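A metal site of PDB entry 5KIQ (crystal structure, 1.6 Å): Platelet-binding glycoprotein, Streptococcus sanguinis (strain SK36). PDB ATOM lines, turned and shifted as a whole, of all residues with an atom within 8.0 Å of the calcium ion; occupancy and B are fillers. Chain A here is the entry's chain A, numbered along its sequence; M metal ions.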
ATOM      1  N   THR A   1      -4.242 -13.989 -16.332  1.00  0.00           N
ATOM      2  CA  THR A   1      -5.596 -14.536 -16.324  1.00  0.00           C
ATOM      3  C   THR A   1      -6.004 -15.131 -17.682  1.00  0.00           C
ATOM      4  O   THR A   1      -5.510 -14.754 -18.739  1.00  0.00           O
ATOM      5  CB  THR A   1      -6.633 -13.460 -15.922  1.00  0.00           C
ATOM      6  OG1 THR A   1      -6.494 -12.321 -16.778  1.00  0.00           O
ATOM      7  CG2 THR A   1      -6.446 -13.039 -14.482  1.00  0.00           C
ATOM      8  N   ASP A   2      -6.909 -16.088 -17.607  1.00  0.00           N
ATOM      9  CA  ASP A   2      -7.450 -16.748 -18.791  1.00  0.00           C
ATOM     10  C   ASP A   2      -8.591 -15.914 -19.336  1.00  0.00           C
ATOM     11  O   ASP A   2      -9.613 -15.723 -18.646  1.00  0.00           O
ATOM     12  CB  ASP A   2      -7.915 -18.140 -18.400  1.00  0.00           C
ATOM     13  CG  ASP A   2      -8.428 -18.974 -19.597  1.00  0.00           C
ATOM     14  OD1 ASP A   2      -8.654 -18.443 -20.715  1.00  0.00           O
ATOM     15  OD2 ASP A   2      -8.568 -20.196 -19.423  1.00  0.00           O
ATOM     16  N   THR A   3      -8.428 -15.437 -20.574  1.00  0.00           N
ATOM     17  CA  THR A   3      -9.428 -14.641 -21.247  1.00  0.00           C
ATOM     18  C   THR A   3      -9.861 -15.289 -22.583  1.00  0.00           C
ATOM     19  O   THR A   3     -10.574 -14.692 -23.375  1.00  0.00           O
ATOM     20  CB  THR A   3      -8.919 -13.216 -21.552  1.00  0.00           C
ATOM     21  OG1 THR A   3      -7.816 -13.295 -22.460  1.00  0.00           O
ATOM     22  CG2 THR A   3      -8.490 -12.503 -20.244  1.00  0.00           C
ATOM     23  N   THR A   4      -9.378 -16.481 -22.857  1.00  0.00           N
ATOM     24  CA  THR A   4      -9.587 -17.091 -24.176  1.00  0.00           C
ATOM     25  C   THR A   4     -10.606 -18.226 -24.064  1.00  0.00           C
ATOM     26  O   THR A   4     -10.421 -19.143 -23.285  1.00  0.00           O
ATOM     27  CB  THR A   4      -8.241 -17.642 -24.751  1.00  0.00           C
ATOM     28  OG1 THR A   4      -7.268 -16.567 -24.796  1.00  0.00           O
ATOM     29  CG2 THR A   4      -8.428 -18.245 -26.148  1.00  0.00           C
ATOM     30  N   PRO A   5     -11.701 -18.183 -24.826  1.00  0.00           N
ATOM     31  CA  PRO A   5     -12.598 -19.336 -24.690  1.00  0.00           C
ATOM     32  C   PRO A   5     -12.099 -20.633 -25.353  1.00  0.00           C
ATOM     33  O   PRO A   5     -11.103 -20.648 -26.131  1.00  0.00           O
ATOM     34  CB  PRO A   5     -13.888 -18.828 -25.376  1.00  0.00           C
ATOM     35  CG  PRO A   5     -13.452 -17.823 -26.344  1.00  0.00           C
ATOM     36  CD  PRO A   5     -12.188 -17.176 -25.779  1.00  0.00           C
ATOM     37  N   PRO A   6     -12.803 -21.755 -25.068  1.00  0.00           N
ATOM     38  CA  PRO A   6     -12.468 -23.047 -25.676  1.00  0.00           C
ATOM     39  C   PRO A   6     -12.644 -23.045 -27.209  1.00  0.00           C
ATOM     40  O   PRO A   6     -13.340 -22.195 -27.737  1.00  0.00           O
ATOM     41  CB  PRO A   6     -13.461 -24.018 -25.024  1.00  0.00           C
ATOM     42  CG  PRO A   6     -13.935 -23.363 -23.772  1.00  0.00           C
ATOM     43  CD  PRO A   6     -13.885 -21.869 -24.055  1.00  0.00           C
ATOM     44  N   THR A   7     -12.002 -23.995 -27.881  1.00  0.00           N
ATOM     45  CA  THR A   7     -12.065 -24.171 -29.344  1.00  0.00           C
ATOM     46  C   THR A   7     -12.726 -25.502 -29.663  1.00  0.00           C
ATOM     47  O   THR A   7     -12.276 -26.547 -29.207  1.00  0.00           O
ATOM     48  CB  THR A   7     -10.667 -24.195 -29.976  1.00  0.00           C
ATOM     49  OG1 THR A   7     -10.033 -22.935 -29.802  1.00  0.00           O
ATOM     50  CG2 THR A   7     -10.734 -24.502 -31.459  1.00  0.00           C
ATOM     51  N   THR A  29     -10.942 -28.166 -27.014  1.00  0.00           N
ATOM     52  CA  THR A  29      -9.709 -27.887 -26.262  1.00  0.00           C
ATOM     53  C   THR A  29      -9.825 -26.489 -25.621  1.00  0.00           C
ATOM     54  O   THR A  29     -10.647 -25.686 -26.059  1.00  0.00           O
ATOM     55  CB  THR A  29      -8.445 -27.942 -27.161  1.00  0.00           C
ATOM     56  OG1 THR A  29      -8.466 -26.897 -28.137  1.00  0.00           O
ATOM     57  CG2 THR A  29      -8.305 -29.269 -27.852  1.00  0.00           C
ATOM     58  N   ASP A  30      -9.066 -26.221 -24.563  1.00  0.00           N
ATOM     59  CA  ASP A  30      -8.942 -24.888 -23.990  1.00  0.00           C
ATOM     60  C   ASP A  30      -7.506 -24.669 -23.572  1.00  0.00           C
ATOM     61  O   ASP A  30      -6.813 -25.634 -23.169  1.00  0.00           O
ATOM     62  CB  ASP A  30      -9.848 -24.677 -22.769  1.00  0.00           C
ATOM     63  CG  ASP A  30      -9.853 -23.217 -22.290  1.00  0.00           C
ATOM     64  OD1 ASP A  30     -10.378 -22.334 -22.986  1.00  0.00           O
ATOM     65  OD2 ASP A  30      -9.328 -22.871 -21.190  1.00  0.00           O
ATOM     66  N   ASP A  31      -7.065 -23.424 -23.619  1.00  0.00           N
ATOM     67  CA  ASP A  31      -5.690 -23.148 -23.238  1.00  0.00           C
ATOM     68  C   ASP A  31      -5.405 -23.519 -21.772  1.00  0.00           C
ATOM     69  O   ASP A  31      -4.266 -23.834 -21.437  1.00  0.00           O
ATOM     70  CB  ASP A  31      -5.326 -21.681 -23.526  1.00  0.00           C
ATOM     71  CG  ASP A  31      -6.231 -20.637 -22.809  1.00  0.00           C
ATOM     72  OD1 ASP A  31      -7.446 -20.851 -22.620  1.00  0.00           O
ATOM     73  OD2 ASP A  31      -5.708 -19.540 -22.474  1.00  0.00           O
ATOM     74  N   SER A  32      -6.414 -23.455 -20.896  1.00  0.00           N
ATOM     75  CA  SER A  32      -6.292 -23.817 -19.475  1.00  0.00           C
ATOM     76  C   SER A  32      -6.241 -25.308 -19.275  1.00  0.00           C
ATOM     77  O   SER A  32      -5.877 -25.784 -18.195  1.00  0.00           O
ATOM     78  CB  SER A  32      -7.459 -23.270 -18.649  1.00  0.00           C
ATOM     79  OG  SER A  32      -8.656 -24.038 -18.877  1.00  0.00           O
ATOM     80  N   GLY A  33      -6.659 -26.043 -20.313  1.00  0.00           N
ATOM     81  CA  GLY A  33      -6.809 -27.477 -20.235  1.00  0.00           C
ATOM     82  C   GLY A  33      -8.079 -27.996 -19.561  1.00  0.00           C
ATOM     83  O   GLY A  33      -8.199 -29.206 -19.414  1.00  0.00           O
ATOM     84  N   GLN A  34      -8.989 -27.103 -19.140  1.00  0.00           N
ATOM     85  CA  GLN A  34     -10.228 -27.474 -18.451  1.00  0.00           C
ATOM     86  C   GLN A  34     -11.445 -26.824 -19.106  1.00  0.00           C
ATOM     87  O   GLN A  34     -11.504 -25.612 -19.199  1.00  0.00           O
ATOM     88  CB  GLN A  34     -10.214 -27.047 -16.967  1.00  0.00           C
ATOM     89  CG  GLN A  34     -11.409 -27.560 -16.129  1.00  0.00           C
ATOM     90  CD  GLN A  34     -11.267 -27.316 -14.626  1.00  0.00           C
ATOM     91  OE1 GLN A  34     -10.180 -27.011 -14.131  1.00  0.00           O
ATOM     92  NE2 GLN A  34     -12.381 -27.407 -13.896  1.00  0.00           N
ATOM     93  N   VAL A  35     -12.407 -27.643 -19.528  1.00  0.00           N
ATOM     94  CA  VAL A  35     -13.697 -27.184 -20.042  1.00  0.00           C
ATOM     95  C   VAL A  35     -14.756 -27.510 -18.970  1.00  0.00           C
ATOM     96  O   VAL A  35     -14.798 -28.623 -18.447  1.00  0.00           O
ATOM     97  CB  VAL A  35     -13.993 -27.844 -21.409  1.00  0.00           C
ATOM     98  CG1 VAL A  35     -15.466 -27.696 -21.811  1.00  0.00           C
ATOM     99  CG2 VAL A  35     -13.122 -27.195 -22.507  1.00  0.00           C
ATOM    100  N   TRP A 101     -17.906 -23.420 -22.199  1.00  0.00           N
ATOM    101  CA  TRP A 101     -17.298 -22.575 -21.154  1.00  0.00           C
ATOM    102  C   TRP A 101     -16.025 -23.195 -20.617  1.00  0.00           C
ATOM    103  O   TRP A 101     -15.960 -24.422 -20.398  1.00  0.00           O
ATOM    104  CB  TRP A 101     -18.211 -22.371 -19.930  1.00  0.00           C
ATOM    105  CG  TRP A 101     -19.390 -21.433 -20.064  1.00  0.00           C
ATOM    106  CD1 TRP A 101     -19.508 -20.167 -19.552  1.00  0.00           C
ATOM    107  CD2 TRP A 101     -20.639 -21.717 -20.717  1.00  0.00           C
ATOM    108  NE1 TRP A 101     -20.749 -19.647 -19.860  1.00  0.00           N
ATOM    109  CE2 TRP A 101     -21.457 -20.559 -20.577  1.00  0.00           C
ATOM    110  CE3 TRP A 101     -21.149 -22.811 -21.390  1.00  0.00           C
ATOM    111  CZ2 TRP A 101     -22.771 -20.508 -21.104  1.00  0.00           C
ATOM    112  CZ3 TRP A 101     -22.449 -22.746 -21.922  1.00  0.00           C
ATOM    113  CH2 TRP A 101     -23.224 -21.598 -21.776  1.00  0.00           C
ATOM    114  N   ASP A 102     -15.041 -22.351 -20.302  1.00  0.00           N
ATOM    115  CA  ASP A 102     -13.916 -22.866 -19.513  1.00  0.00           C
ATOM    116  C   ASP A 102     -14.208 -22.603 -18.020  1.00  0.00           C
ATOM    117  O   ASP A 102     -15.310 -22.208 -17.670  1.00  0.00           O
ATOM    118  CB  ASP A 102     -12.578 -22.256 -20.004  1.00  0.00           C
ATOM    119  CG  ASP A 102     -12.476 -20.740 -19.793  1.00  0.00           C
ATOM    120  OD1 ASP A 102     -13.241 -20.162 -18.980  1.00  0.00           O
ATOM    121  OD2 ASP A 102     -11.609 -20.147 -20.477  1.00  0.00           O
ATOM    122  N   ALA A 103     -13.259 -22.887 -17.131  1.00  0.00           N
ATOM    123  CA  ALA A 103     -13.507 -22.702 -15.700  1.00  0.00           C
ATOM    124  C   ALA A 103     -13.339 -21.278 -15.229  1.00  0.00           C
ATOM    125  O   ALA A 103     -13.577 -20.988 -14.060  1.00  0.00           O
ATOM    126  CB  ALA A 103     -12.585 -23.617 -14.894  1.00  0.00           C
ATOM    127  N   ALA A 104     -12.960 -20.381 -16.132  1.00  0.00           N
ATOM    128  CA  ALA A 104     -12.752 -18.977 -15.803  1.00  0.00           C
ATOM    129  C   ALA A 104     -13.894 -18.067 -16.260  1.00  0.00           C
ATOM    130  O   ALA A 104     -13.764 -16.846 -16.238  1.00  0.00           O
ATOM    131  CB  ALA A 104     -11.458 -18.499 -16.415  1.00  0.00           C
ATOM    132  N   GLY A 105     -14.985 -18.672 -16.737  1.00  0.00           N
ATOM    133  CA  GLY A 105     -16.124 -17.896 -17.202  1.00  0.00           C
ATOM    134  C   GLY A 105     -16.099 -17.485 -18.658  1.00  0.00           C
ATOM    135  O   GLY A 105     -16.992 -16.762 -19.110  1.00  0.00           O
ATOM    136  N   ASN A 106     -15.080 -17.895 -19.409  1.00  0.00           N
ATOM    137  CA  ASN A 106     -15.048 -17.582 -20.845  1.00  0.00           C
ATOM    138  C   ASN A 106     -15.877 -18.550 -21.675  1.00  0.00           C
ATOM    139  O   ASN A 106     -15.632 -19.762 -21.648  1.00  0.00           O
ATOM    140  CB  ASN A 106     -13.625 -17.591 -21.374  1.00  0.00           C
ATOM    141  CG  ASN A 106     -12.727 -16.681 -20.602  1.00  0.00           C
ATOM    142  OD1 ASN A 106     -12.931 -15.459 -20.577  1.00  0.00           O
ATOM    143  ND2 ASN A 106     -11.707 -17.253 -20.001  1.00  0.00           N
ATOM    144  N   VAL A 107     -16.805 -18.024 -22.469  1.00  0.00           N
ATOM    145  CA  VAL A 107     -17.605 -18.892 -23.340  1.00  0.00           C
ATOM    146  C   VAL A 107     -17.333 -18.645 -24.844  1.00  0.00           C
ATOM    147  O   VAL A 107     -17.087 -17.527 -25.261  1.00  0.00           O
ATOM    148  CB  VAL A 107     -19.085 -18.736 -23.018  1.00  0.00           C
ATOM    149  CG1 VAL A 107     -19.581 -17.342 -23.298  1.00  0.00           C
ATOM    150  CG2 VAL A 107     -19.926 -19.746 -23.798  1.00  0.00           C
HETATM  151 CA    CA M   1      -9.529 -20.516 -21.579  1.00  0.00          CA
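The side-chain carboxylate of Asp 102 sits at hydrogen-bond distance from the backbone NH of Asn 106 (3.0 Å).
The backbone NH of Ala 104 is in hydrogen-bond range of the side-chain carboxylate of Asp 102, at 2.9 Å.
The backbone carbonyl oxygen (O) of Asp 2 is in hydrogen-bond range of the side-chain amide nitrogen (ND2) of Asn 106 (2.9 Å).
The side-chain carboxylate (OD2) of Asp 30 sits close to the side-chain hydroxyl (OG) of Ser 32, 2.7 Å away.
N of Gly 105 sits at hydrogen-bond distance from OD1 of Asp 102 (3.2 Å).
Of the 21 residues printed, 5 come within 4 Å of the calcium ion.
The nearest printed residue that does not touch the calcium ion is Asn 106 (4.2 Å).
OD1 of Asp 31 binds the calcium ion (2.4 Å).
O of Thr 4 binds the calcium ion, 2.4 Å away.
The calcium ion is bound by OD2 of Asp 2, 2.4 Å away.
The side-chain carboxylate (OD2) of Asp 102 binds the calcium ion (2.4 Å).
The calcium ion is bound by OD2 of Asp 30, at 2.4 Å.
OD1 of Asp 2 is bound to the calcium ion (2.4 Å).
OD1 of Asp 30 binds the calcium ion (2.5 Å).
The calcium ion has seven donor atoms within binding distance.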
